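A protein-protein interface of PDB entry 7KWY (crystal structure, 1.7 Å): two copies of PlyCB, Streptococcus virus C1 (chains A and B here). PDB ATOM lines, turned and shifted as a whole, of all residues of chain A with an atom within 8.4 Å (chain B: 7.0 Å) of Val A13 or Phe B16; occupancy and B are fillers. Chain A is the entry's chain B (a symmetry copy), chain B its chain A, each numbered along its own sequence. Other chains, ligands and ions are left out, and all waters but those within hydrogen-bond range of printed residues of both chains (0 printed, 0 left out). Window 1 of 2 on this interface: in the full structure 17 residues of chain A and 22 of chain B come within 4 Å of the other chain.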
ATOM      1  N   ASN A   9       0.252 -29.037 -17.645  1.00  0.00           N
ATOM      2  CA  ASN A   9       1.659 -28.661 -17.551  1.00  0.00           C
ATOM      3  C   ASN A   9       1.969 -28.399 -16.091  1.00  0.00           C
ATOM      4  O   ASN A   9       1.966 -27.263 -15.605  1.00  0.00           O
ATOM      5  CB  ASN A   9       1.997 -27.466 -18.422  1.00  0.00           C
ATOM      6  CG  ASN A   9       3.493 -27.302 -18.600  1.00  0.00           C
ATOM      7  OD1 ASN A   9       3.947 -26.314 -19.173  1.00  0.00           O
ATOM      8  ND2 ASN A   9       4.271 -28.279 -18.116  1.00  0.00           N
ATOM      9  N   VAL A  10       2.253 -29.500 -15.403  1.00  0.00           N
ATOM     10  CA  VAL A  10       2.664 -29.517 -14.026  1.00  0.00           C
ATOM     11  C   VAL A  10       3.858 -28.601 -13.734  1.00  0.00           C
ATOM     12  O   VAL A  10       4.038 -28.192 -12.585  1.00  0.00           O
ATOM     13  CB  VAL A  10       2.964 -30.987 -13.708  1.00  0.00           C
ATOM     14  CG1 VAL A  10       3.964 -31.518 -14.748  1.00  0.00           C
ATOM     15  CG2 VAL A  10       3.470 -31.141 -12.350  1.00  0.00           C
ATOM     16  N   SER A  11       4.683 -28.284 -14.724  1.00  0.00           N
ATOM     17  CA  SER A  11       5.912 -27.550 -14.382  1.00  0.00           C
ATOM     18  C   SER A  11       5.683 -26.055 -14.211  1.00  0.00           C
ATOM     19  O   SER A  11       6.527 -25.372 -13.628  1.00  0.00           O
ATOM     20  CB  SER A  11       6.977 -27.743 -15.455  1.00  0.00           C
ATOM     21  OG  SER A  11       6.634 -26.965 -16.578  1.00  0.00           O
ATOM     22  N   GLY A  12       4.577 -25.528 -14.731  1.00  0.00           N
ATOM     23  CA  GLY A  12       4.365 -24.109 -14.608  1.00  0.00           C
ATOM     24  C   GLY A  12       5.257 -23.298 -15.517  1.00  0.00           C
ATOM     25  O   GLY A  12       5.385 -22.095 -15.325  1.00  0.00           O
ATOM     26  N   VAL A  13       5.872 -23.927 -16.508  1.00  0.00           N
ATOM     27  CA  VAL A  13       6.733 -23.248 -17.473  1.00  0.00           C
ATOM     28  C   VAL A  13       6.206 -23.509 -18.871  1.00  0.00           C
ATOM     29  O   VAL A  13       6.036 -24.669 -19.258  1.00  0.00           O
ATOM     30  CB  VAL A  13       8.164 -23.762 -17.375  1.00  0.00           C
ATOM     31  CG1 VAL A  13       9.070 -22.982 -18.371  1.00  0.00           C
ATOM     32  CG2 VAL A  13       8.666 -23.611 -15.921  1.00  0.00           C
ATOM     33  N   GLN A  14       5.987 -22.446 -19.642  1.00  0.00           N
ATOM     34  CA  GLN A  14       5.752 -22.567 -21.074  1.00  0.00           C
ATOM     35  C   GLN A  14       6.819 -21.786 -21.807  1.00  0.00           C
ATOM     36  O   GLN A  14       7.067 -20.633 -21.445  1.00  0.00           O
ATOM     37  CB  GLN A  14       4.420 -21.982 -21.464  1.00  0.00           C
ATOM     38  CG  GLN A  14       3.351 -22.974 -21.473  1.00  0.00           C
ATOM     39  CD  GLN A  14       2.179 -22.473 -22.253  1.00  0.00           C
ATOM     40  OE1 GLN A  14       2.073 -21.286 -22.483  1.00  0.00           O
ATOM     41  NE2 GLN A  14       1.288 -23.373 -22.658  1.00  0.00           N
ATOM     42  N   GLY A  15       7.439 -22.397 -22.822  1.00  0.00           N
ATOM     43  CA  GLY A  15       8.442 -21.724 -23.636  1.00  0.00           C
ATOM     44  C   GLY A  15       9.446 -22.703 -24.220  1.00  0.00           C
ATOM     45  O   GLY A  15       9.157 -23.889 -24.393  1.00  0.00           O
ATOM     46  N   PHE A  16      10.627 -22.174 -24.565  1.00  0.00           N
ATOM     47  CA  PHE A  16      11.613 -22.978 -25.266  1.00  0.00           C
ATOM     48  C   PHE A  16      12.980 -22.326 -25.102  1.00  0.00           C
ATOM     49  O   PHE A  16      13.094 -21.112 -24.919  1.00  0.00           O
ATOM     50  CB  PHE A  16      11.270 -23.142 -26.769  1.00  0.00           C
ATOM     51  CG  PHE A  16      11.125 -21.841 -27.526  1.00  0.00           C
ATOM     52  CD1 PHE A  16       9.901 -21.176 -27.553  1.00  0.00           C
ATOM     53  CD2 PHE A  16      12.203 -21.299 -28.222  1.00  0.00           C
ATOM     54  CE1 PHE A  16       9.756 -19.995 -28.270  1.00  0.00           C
ATOM     55  CE2 PHE A  16      12.070 -20.104 -28.933  1.00  0.00           C
ATOM     56  CZ  PHE A  16      10.843 -19.458 -28.962  1.00  0.00           C
ATOM     57  N   ALA A  30      16.322 -18.325 -23.595  1.00  0.00           N
ATOM     58  CA  ALA A  30      15.038 -19.011 -23.461  1.00  0.00           C
ATOM     59  C   ALA A  30      13.927 -17.994 -23.376  1.00  0.00           C
ATOM     60  O   ALA A  30      14.126 -16.883 -22.884  1.00  0.00           O
ATOM     61  CB  ALA A  30      14.969 -19.893 -22.204  1.00  0.00           C
ATOM     62  N   PHE A  31      12.745 -18.399 -23.845  1.00  0.00           N
ATOM     63  CA  PHE A  31      11.506 -17.715 -23.509  1.00  0.00           C
ATOM     64  C   PHE A  31      10.845 -18.572 -22.452  1.00  0.00           C
ATOM     65  O   PHE A  31      10.610 -19.756 -22.696  1.00  0.00           O
ATOM     66  CB  PHE A  31      10.587 -17.581 -24.720  1.00  0.00           C
ATOM     67  CG  PHE A  31      11.005 -16.512 -25.650  1.00  0.00           C
ATOM     68  CD1 PHE A  31      10.715 -15.188 -25.368  1.00  0.00           C
ATOM     69  CD2 PHE A  31      11.699 -16.818 -26.809  1.00  0.00           C
ATOM     70  CE1 PHE A  31      11.126 -14.187 -26.234  1.00  0.00           C
ATOM     71  CE2 PHE A  31      12.109 -15.821 -27.680  1.00  0.00           C
ATOM     72  CZ  PHE A  31      11.825 -14.509 -27.385  1.00  0.00           C
ATOM     73  N   ILE A  32      10.622 -17.994 -21.283  1.00  0.00           N
ATOM     74  CA  ILE A  32       9.976 -18.657 -20.155  1.00  0.00           C
ATOM     75  C   ILE A  32       8.760 -17.828 -19.790  1.00  0.00           C
ATOM     76  O   ILE A  32       8.903 -16.688 -19.323  1.00  0.00           O
ATOM     77  CB  ILE A  32      10.926 -18.769 -18.955  1.00  0.00           C
ATOM     78  CG1 ILE A  32      12.244 -19.466 -19.342  1.00  0.00           C
ATOM     79  CG2 ILE A  32      10.178 -19.355 -17.710  1.00  0.00           C
ATOM     80  CD1 ILE A  32      12.176 -20.947 -19.387  1.00  0.00           C
ATOM     81  N   ASN A  33       7.558 -18.384 -19.994  1.00  0.00           N
ATOM     82  CA  ASN A  33       6.319 -17.689 -19.671  1.00  0.00           C
ATOM     83  C   ASN A  33       6.305 -16.269 -20.245  1.00  0.00           C
ATOM     84  O   ASN A  33       5.959 -15.294 -19.568  1.00  0.00           O
ATOM     85  CB  ASN A  33       6.100 -17.709 -18.158  1.00  0.00           C
ATOM     86  CG  ASN A  33       5.991 -19.130 -17.624  1.00  0.00           C
ATOM     87  OD1 ASN A  33       5.653 -20.044 -18.386  1.00  0.00           O
ATOM     88  ND2 ASN A  33       6.252 -19.325 -16.332  1.00  0.00           N
ATOM     89  N   GLY A  34       6.729 -16.170 -21.505  1.00  0.00           N
ATOM     90  CA  GLY A  34       6.717 -14.933 -22.259  1.00  0.00           C
ATOM     91  C   GLY A  34       7.825 -13.964 -21.923  1.00  0.00           C
ATOM     92  O   GLY A  34       7.774 -12.809 -22.367  1.00  0.00           O
ATOM     93  N   GLY A  47      19.012 -28.873 -17.556  1.00  0.00           N
ATOM     94  CA  GLY A  47      17.882 -28.896 -16.632  1.00  0.00           C
ATOM     95  C   GLY A  47      16.600 -28.508 -17.339  1.00  0.00           C
ATOM     96  O   GLY A  47      15.604 -29.238 -17.285  1.00  0.00           O
ATOM     97  N   PHE A  48      16.603 -27.357 -18.014  1.00  0.00           N
ATOM     98  CA  PHE A  48      15.361 -26.969 -18.701  1.00  0.00           C
ATOM     99  C   PHE A  48      15.029 -27.859 -19.881  1.00  0.00           C
ATOM    100  O   PHE A  48      13.845 -27.968 -20.228  1.00  0.00           O
ATOM    101  CB  PHE A  48      15.413 -25.500 -19.132  1.00  0.00           C
ATOM    102  CG  PHE A  48      15.012 -24.581 -17.999  1.00  0.00           C
ATOM    103  CD1 PHE A  48      13.683 -24.325 -17.751  1.00  0.00           C
ATOM    104  CD2 PHE A  48      15.951 -24.112 -17.108  1.00  0.00           C
ATOM    105  CE1 PHE A  48      13.277 -23.540 -16.667  1.00  0.00           C
ATOM    106  CE2 PHE A  48      15.573 -23.323 -16.024  1.00  0.00           C
ATOM    107  CZ  PHE A  48      14.213 -23.047 -15.802  1.00  0.00           C
ATOM    108  N   ILE A  51      12.125 -30.204 -19.416  1.00  0.00           N
ATOM    109  CA  ILE A  51      10.733 -29.748 -19.299  1.00  0.00           C
ATOM    110  C   ILE A  51      10.272 -28.827 -20.426  1.00  0.00           C
ATOM    111  O   ILE A  51       9.042 -28.588 -20.534  1.00  0.00           O
ATOM    112  CB  ILE A  51      10.487 -29.059 -17.941  1.00  0.00           C
ATOM    113  CG1 ILE A  51      11.392 -27.834 -17.742  1.00  0.00           C
ATOM    114  CG2 ILE A  51      10.623 -30.015 -16.753  1.00  0.00           C
ATOM    115  CD1 ILE A  51      10.913 -26.921 -16.576  1.00  0.00           C
ATOM    116  N   ILE A  52      11.155 -28.231 -21.226  1.00  0.00           N
ATOM    117  CA  ILE A  52      10.726 -27.445 -22.386  1.00  0.00           C
ATOM    118  C   ILE A  52      11.568 -27.831 -23.600  1.00  0.00           C
ATOM    119  O   ILE A  52      12.704 -28.324 -23.488  1.00  0.00           O
ATOM    120  CB  ILE A  52      10.809 -25.921 -22.125  1.00  0.00           C
ATOM    121  CG1 ILE A  52      12.217 -25.519 -21.639  1.00  0.00           C
ATOM    122  CG2 ILE A  52       9.771 -25.469 -21.129  1.00  0.00           C
ATOM    123  CD1 ILE A  52      12.365 -24.030 -21.525  1.00  0.00           C
ATOM    124  N   PRO A  53      11.036 -27.592 -24.792  1.00  0.00           N
ATOM    125  CA  PRO A  53      11.805 -27.905 -26.000  1.00  0.00           C
ATOM    126  C   PRO A  53      12.997 -26.985 -26.187  1.00  0.00           C
ATOM    127  O   PRO A  53      13.047 -25.851 -25.687  1.00  0.00           O
ATOM    128  CB  PRO A  53      10.796 -27.684 -27.146  1.00  0.00           C
ATOM    129  CG  PRO A  53       9.717 -26.858 -26.556  1.00  0.00           C
ATOM    130  CD  PRO A  53       9.641 -27.209 -25.074  1.00  0.00           C
ATOM    131  N   VAL B  13      -0.870 -28.006  -7.971  1.00  0.00           N
ATOM    132  CA  VAL B  13       0.481 -27.456  -7.804  1.00  0.00           C
ATOM    133  C   VAL B  13       1.149 -27.411  -9.160  1.00  0.00           C
ATOM    134  O   VAL B  13       1.201 -28.435  -9.848  1.00  0.00           O
ATOM    135  CB  VAL B  13       1.334 -28.311  -6.865  1.00  0.00           C
ATOM    136  CG1 VAL B  13       2.763 -27.738  -6.832  1.00  0.00           C
ATOM    137  CG2 VAL B  13       0.760 -28.366  -5.427  1.00  0.00           C
ATOM    138  N   GLN B  14       1.671 -26.242  -9.546  1.00  0.00           N
ATOM    139  CA  GLN B  14       2.472 -26.111 -10.757  1.00  0.00           C
ATOM    140  C   GLN B  14       3.824 -25.555 -10.364  1.00  0.00           C
ATOM    141  O   GLN B  14       3.892 -24.573  -9.611  1.00  0.00           O
ATOM    142  CB  GLN B  14       1.849 -25.168 -11.774  1.00  0.00           C
ATOM    143  CG  GLN B  14       0.566 -25.661 -12.338  1.00  0.00           C
ATOM    144  CD  GLN B  14       0.163 -24.777 -13.492  1.00  0.00           C
ATOM    145  OE1 GLN B  14       0.034 -25.236 -14.618  1.00  0.00           O
ATOM    146  NE2 GLN B  14       0.012 -23.489 -13.222  1.00  0.00           N
ATOM    147  N   GLY B  15       4.890 -26.180 -10.849  1.00  0.00           N
ATOM    148  CA  GLY B  15       6.206 -25.649 -10.504  1.00  0.00           C
ATOM    149  C   GLY B  15       7.262 -26.730 -10.615  1.00  0.00           C
ATOM    150  O   GLY B  15       7.070 -27.731 -11.280  1.00  0.00           O
ATOM    151  N   PHE B  16       8.394 -26.488  -9.973  1.00  0.00           N
ATOM    152  CA  PHE B  16       9.450 -27.487 -10.045  1.00  0.00           C
ATOM    153  C   PHE B  16      10.417 -27.250  -8.895  1.00  0.00           C
ATOM    154  O   PHE B  16      10.503 -26.146  -8.351  1.00  0.00           O
ATOM    155  CB  PHE B  16      10.194 -27.453 -11.408  1.00  0.00           C
ATOM    156  CG  PHE B  16      10.777 -26.087 -11.756  1.00  0.00           C
ATOM    157  CD1 PHE B  16      12.034 -25.692 -11.287  1.00  0.00           C
ATOM    158  CD2 PHE B  16      10.053 -25.204 -12.549  1.00  0.00           C
ATOM    159  CE1 PHE B  16      12.533 -24.436 -11.593  1.00  0.00           C
ATOM    160  CE2 PHE B  16      10.563 -23.951 -12.892  1.00  0.00           C
ATOM    161  CZ  PHE B  16      11.819 -23.575 -12.386  1.00  0.00           C
ATOM    162  N   LEU B  17      11.119 -28.313  -8.533  1.00  0.00           N
ATOM    163  CA  LEU B  17      12.265 -28.273  -7.631  1.00  0.00           C
ATOM    164  C   LEU B  17      13.514 -27.939  -8.438  1.00  0.00           C
ATOM    165  O   LEU B  17      13.621 -28.298  -9.627  1.00  0.00           O
ATOM    166  CB  LEU B  17      12.453 -29.633  -6.952  1.00  0.00           C
ATOM    167  CG  LEU B  17      11.409 -30.077  -5.897  1.00  0.00           C
ATOM    168  CD1 LEU B  17      11.300 -31.576  -5.869  1.00  0.00           C
ATOM    169  CD2 LEU B  17      11.937 -29.606  -4.579  1.00  0.00           C
ATOM    170  N   PHE B  18      14.457 -27.244  -7.793  1.00  0.00           N
ATOM    171  CA  PHE B  18      15.715 -26.991  -8.487  1.00  0.00           C
ATOM    172  C   PHE B  18      16.872 -27.010  -7.505  1.00  0.00           C
ATOM    173  O   PHE B  18      16.730 -26.612  -6.346  1.00  0.00           O
ATOM    174  CB  PHE B  18      15.734 -25.667  -9.284  1.00  0.00           C
ATOM    175  CG  PHE B  18      15.386 -24.390  -8.514  1.00  0.00           C
ATOM    176  CD1 PHE B  18      14.046 -24.061  -8.228  1.00  0.00           C
ATOM    177  CD2 PHE B  18      16.381 -23.458  -8.199  1.00  0.00           C
ATOM    178  CE1 PHE B  18      13.741 -22.858  -7.563  1.00  0.00           C
ATOM    179  CE2 PHE B  18      16.093 -22.271  -7.559  1.00  0.00           C
ATOM    180  CZ  PHE B  18      14.742 -21.967  -7.232  1.00  0.00           C
ATOM    181  N   ARG B  29      15.625 -25.867  -3.725  1.00  0.00           N
ATOM    182  CA  ARG B  29      14.592 -24.830  -3.675  1.00  0.00           C
ATOM    183  C   ARG B  29      13.446 -25.256  -4.582  1.00  0.00           C
ATOM    184  O   ARG B  29      13.535 -26.265  -5.278  1.00  0.00           O
ATOM    185  CB  ARG B  29      15.138 -23.469  -4.109  1.00  0.00           C
ATOM    186  CG  ARG B  29      16.330 -23.011  -3.186  1.00  0.00           C
ATOM    187  CD  ARG B  29      16.825 -21.608  -3.474  1.00  0.00           C
ATOM    188  NE  ARG B  29      15.877 -20.558  -3.086  1.00  0.00           N
ATOM    189  CZ  ARG B  29      15.682 -20.110  -1.844  1.00  0.00           C
ATOM    190  NH1 ARG B  29      16.365 -20.625  -0.812  1.00  0.00           N
ATOM    191  NH2 ARG B  29      14.791 -19.138  -1.628  1.00  0.00           N
ATOM    192  N   ALA B  30      12.361 -24.483  -4.587  1.00  0.00           N
ATOM    193  CA  ALA B  30      11.275 -24.823  -5.514  1.00  0.00           C
ATOM    194  C   ALA B  30      10.512 -23.572  -5.911  1.00  0.00           C
ATOM    195  O   ALA B  30      10.553 -22.557  -5.222  1.00  0.00           O
ATOM    196  CB  ALA B  30      10.302 -25.843  -4.893  1.00  0.00           C
ATOM    197  N   PHE B  31       9.849 -23.634  -7.073  1.00  0.00           N
ATOM    198  CA  PHE B  31       8.765 -22.721  -7.407  1.00  0.00           C
ATOM    199  C   PHE B  31       7.486 -23.512  -7.238  1.00  0.00           C
ATOM    200  O   PHE B  31       7.380 -24.615  -7.772  1.00  0.00           O
ATOM    201  CB  PHE B  31       8.883 -22.203  -8.847  1.00  0.00           C
ATOM    202  CG  PHE B  31       9.976 -21.212  -9.022  1.00  0.00           C
ATOM    203  CD1 PHE B  31       9.789 -19.897  -8.663  1.00  0.00           C
ATOM    204  CD2 PHE B  31      11.207 -21.607  -9.517  1.00  0.00           C
ATOM    205  CE1 PHE B  31      10.843 -18.985  -8.800  1.00  0.00           C
ATOM    206  CE2 PHE B  31      12.272 -20.679  -9.656  1.00  0.00           C
ATOM    207  CZ  PHE B  31      12.074 -19.391  -9.291  1.00  0.00           C
ATOM    208  N   ILE B  32       6.560 -22.989  -6.430  1.00  0.00           N
ATOM    209  CA  ILE B  32       5.273 -23.631  -6.152  1.00  0.00           C
ATOM    210  C   ILE B  32       4.229 -22.574  -6.450  1.00  0.00           C
ATOM    211  O   ILE B  32       4.140 -21.578  -5.726  1.00  0.00           O
ATOM    212  CB  ILE B  32       5.150 -24.096  -4.688  1.00  0.00           C
ATOM    213  CG1 ILE B  32       6.259 -25.070  -4.294  1.00  0.00           C
ATOM    214  CG2 ILE B  32       3.764 -24.777  -4.448  1.00  0.00           C
ATOM    215  CD1 ILE B  32       6.104 -26.412  -4.925  1.00  0.00           C
ATOM    216  N   ASN B  33       3.458 -22.767  -7.525  1.00  0.00           N
ATOM    217  CA  ASN B  33       2.443 -21.805  -7.923  1.00  0.00           C
ATOM    218  C   ASN B  33       2.998 -20.381  -7.956  1.00  0.00           C
ATOM    219  O   ASN B  33       2.368 -19.435  -7.464  1.00  0.00           O
ATOM    220  CB  ASN B  33       1.238 -21.922  -6.989  1.00  0.00           C
ATOM    221  CG  ASN B  33       0.554 -23.286  -7.103  1.00  0.00           C
ATOM    222  OD1 ASN B  33       0.759 -24.006  -8.087  1.00  0.00           O
ATOM    223  ND2 ASN B  33      -0.258 -23.642  -6.105  1.00  0.00           N
ATOM    224  N   ILE B  52       5.855 -32.890  -8.880  1.00  0.00           N
ATOM    225  CA  ILE B  52       6.381 -31.863  -9.796  1.00  0.00           C
ATOM    226  C   ILE B  52       7.788 -32.245 -10.239  1.00  0.00           C
ATOM    227  O   ILE B  52       8.481 -33.034  -9.583  1.00  0.00           O
ATOM    228  CB  ILE B  52       6.396 -30.446  -9.152  1.00  0.00           C
ATOM    229  CG1 ILE B  52       7.241 -30.384  -7.864  1.00  0.00           C
ATOM    230  CG2 ILE B  52       4.955 -29.974  -8.891  1.00  0.00           C
ATOM    231  CD1 ILE B  52       7.341 -28.960  -7.239  1.00  0.00           C
ATOM    232  N   PRO B  53       8.212 -31.742 -11.395  1.00  0.00           N
ATOM    233  CA  PRO B  53       9.553 -32.081 -11.872  1.00  0.00           C
ATOM    234  C   PRO B  53      10.634 -31.515 -10.974  1.00  0.00           C
ATOM    235  O   PRO B  53      10.434 -30.582 -10.172  1.00  0.00           O
ATOM    236  CB  PRO B  53       9.616 -31.476 -13.283  1.00  0.00           C
ATOM    237  CG  PRO B  53       8.434 -30.549 -13.397  1.00  0.00           C
ATOM    238  CD  PRO B  53       7.410 -30.981 -12.378  1.00  0.00           C
ATOM    239  N   SER B  54      11.810 -32.116 -11.113  1.00  0.00           N
ATOM    240  CA  SER B  54      12.984 -31.688 -10.343  1.00  0.00           C
ATOM    241  C   SER B  54      14.147 -31.546 -11.323  1.00  0.00           C
ATOM    242  O   SER B  54      14.527 -32.516 -11.990  1.00  0.00           O
ATOM    243  CB  SER B  54      13.311 -32.706  -9.243  1.00  0.00           C
ATOM    244  OG  SER B  54      14.488 -32.312  -8.522  1.00  0.00           O
ATOM    245  N   ILE B  55      14.642 -30.328 -11.482  1.00  0.00           N
ATOM    246  CA  ILE B  55      15.628 -30.050 -12.529  1.00  0.00           C
ATOM    247  C   ILE B  55      16.833 -29.372 -11.905  1.00  0.00           C
ATOM    248  O   ILE B  55      16.815 -28.948 -10.752  1.00  0.00           O
ATOM    249  CB  ILE B  55      15.046 -29.173 -13.673  1.00  0.00           C
ATOM    250  CG1 ILE B  55      14.660 -27.790 -13.114  1.00  0.00           C
ATOM    251  CG2 ILE B  55      13.857 -29.891 -14.309  1.00  0.00           C
ATOM    252  CD1 ILE B  55      14.180 -26.769 -14.213  1.00  0.00           C
ATOM    253  N   ILE B  57      19.599 -26.278 -11.980  1.00  0.00           N
ATOM    254  CA  ILE B  57      19.785 -24.876 -12.371  1.00  0.00           C
ATOM    255  C   ILE B  57      21.074 -24.403 -11.728  1.00  0.00           C
ATOM    256  O   ILE B  57      21.214 -24.476 -10.499  1.00  0.00           O
ATOM    257  CB  ILE B  57      18.602 -23.985 -11.923  1.00  0.00           C
ATOM    258  CG1 ILE B  57      17.284 -24.496 -12.531  1.00  0.00           C
ATOM    259  CG2 ILE B  57      18.862 -22.544 -12.317  1.00  0.00           C
ATOM    260  CD1 ILE B  57      16.054 -23.580 -12.202  1.00  0.00           C
ATOM    261  N   ILE B  65      15.955 -16.924 -13.720  1.00  0.00           N
ATOM    262  CA  ILE B  65      14.787 -17.793 -13.707  1.00  0.00           C
ATOM    263  C   ILE B  65      13.728 -17.221 -12.779  1.00  0.00           C
ATOM    264  O   ILE B  65      12.540 -17.278 -13.072  1.00  0.00           O
ATOM    265  CB  ILE B  65      15.150 -19.235 -13.301  1.00  0.00           C
ATOM    266  CG1 ILE B  65      16.186 -19.827 -14.280  1.00  0.00           C
ATOM    267  CG2 ILE B  65      13.885 -20.104 -13.203  1.00  0.00           C
ATOM    268  CD1 ILE B  65      15.688 -19.858 -15.703  1.00  0.00           C
ATOM    269  N   MET B  69       9.819 -16.522 -13.538  1.00  0.00           N
ATOM    270  CA  MET B  69       8.810 -17.221 -12.759  1.00  0.00           C
ATOM    271  C   MET B  69       8.013 -16.282 -11.840  1.00  0.00           C
ATOM    272  O   MET B  69       7.274 -16.763 -10.973  1.00  0.00           O
ATOM    273  CB  MET B  69       9.459 -18.360 -11.954  1.00  0.00           C
ATOM    274  CG  MET B  69      10.095 -19.483 -12.802  1.00  0.00           C
ATOM    275  SD  MET B  69       8.959 -20.396 -13.908  1.00  0.00           S
ATOM    276  CE  MET B  69       7.982 -21.319 -12.720  1.00  0.00           C
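Of the 18 printed residues of chain B, 10 touch a printed residue of chain A.
Hydrophobic or aromatic side chains of chain A within 4 Å of the printed part of chain B: Val A10, Val A13, Phe A48 and Ile A51.
Among the printed residues, 19 pairs touch across the chains.
Among the printed residues, no Asp or Glu carboxylate lies within 4 Å of a Lys or Arg side-chain nitrogen of the other chain.
O of Val A10 touches O of Val B13 (3.9 Å).
O of Val A10 touches CA of Gln B14 (3.2 Å).
CG2 of Val A10 touches CA of Ile B52, 3.9 Å away.
Val A10 touches Pro B53 (CG2 to CD, 3.9 Å).
CD2 of Phe B16 touches O of Ser A11, at 3.7 Å.
CG of Pro B53 touches CB of Ser A11, at 3.8 Å.
Gly A12 touches Gly B15 (N to N, 3.9 Å).
CG2 of Val A13 touches SD of Met B69 (3.8 Å).
CG2 of Ile B55 touches O of Gly A47, 3.5 Å away.
Phe A48 touches Ile B65.
The backbone carbonyl oxygen (O) of Phe B16 is in hydrogen-bond range of the backbone NH (N) of Phe B31 (2.9 Å).
The backbone NH (N) of Leu B17 sits at hydrogen-bond distance from the backbone carbonyl oxygen (O) of Pro B53, 2.9 Å away.
O of Gln A14 lies within hydrogen-bond range of N of Asn A33, at 2.7 Å.
The side-chain amide nitrogen of Asn A9 sits at hydrogen-bond distance from the side-chain hydroxyl of Ser A11, at 3.1 Å.
The backbone NH (N) of Ile B55 lies within hydrogen-bond range of the backbone carbonyl oxygen (O) of Leu B17.
The backbone carbonyl oxygen of Gln B14 sits at hydrogen-bond distance from the backbone NH of Asn B33, at 2.8 Å.
Of chain B, only Gln B14, Gly B15 and Met B69 come within 4 Å of Gly A12.
Of chain B, only Phe B16 and Met B69 come within 4 Å of Val A13.
Ile A32 touches none of the printed residues of chain B.
Printed residues of chain B within 4 Å of Asn A33: Met B69 (3.8 Å).
Printed residues of chain B within 4 Å of Ile A51: Pro B53.
Of chain A, only Val A10, Ser A11 and Gly A12 come within 4 Å of Gly B15.
Phe B16 touches just these residues of chain A: Ser A11 (3.7 Å) and Val A13 (3.6 Å).
Ala B30 touches none of the printed residues of chain A.
Of the printed residues of chain A, Pro B53 touches Val A10, Ser A11 and Ile A51.
The nearest residue of chain B that does not touch Val A13 is Gly B15 (6.2 Å).
The nearest residue of chain A that does not touch Phe B16 is Phe A48 (4.2 Å).
The nearest printed residue of chain B that does not touch Asn A9 is Gly B15 (5.7 Å).
SD of Met B69 sits at hydrogen-bond distance from ND2 of Asn A33, at 3.8 Å.
N of Gly B15 sits close to O of Ser A11 (3.3 Å).
The side-chain amide oxygen of Gln B14 sits close to the backbone carbonyl oxygen of Asn A9, at 3.0 Å.
The backbone NH (N) of Gly B15 lies within hydrogen-bond range of the backbone carbonyl oxygen (O) of Val A10 (2.8 Å).
Val A13 touches Phe B16, but with the chains exchanged Phe A16 does not touch Val B13 (18.6 Å).
Positions printed for both chains: 13, 14, 15, 16, 30, 31, 32, 33, 52 and 53.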
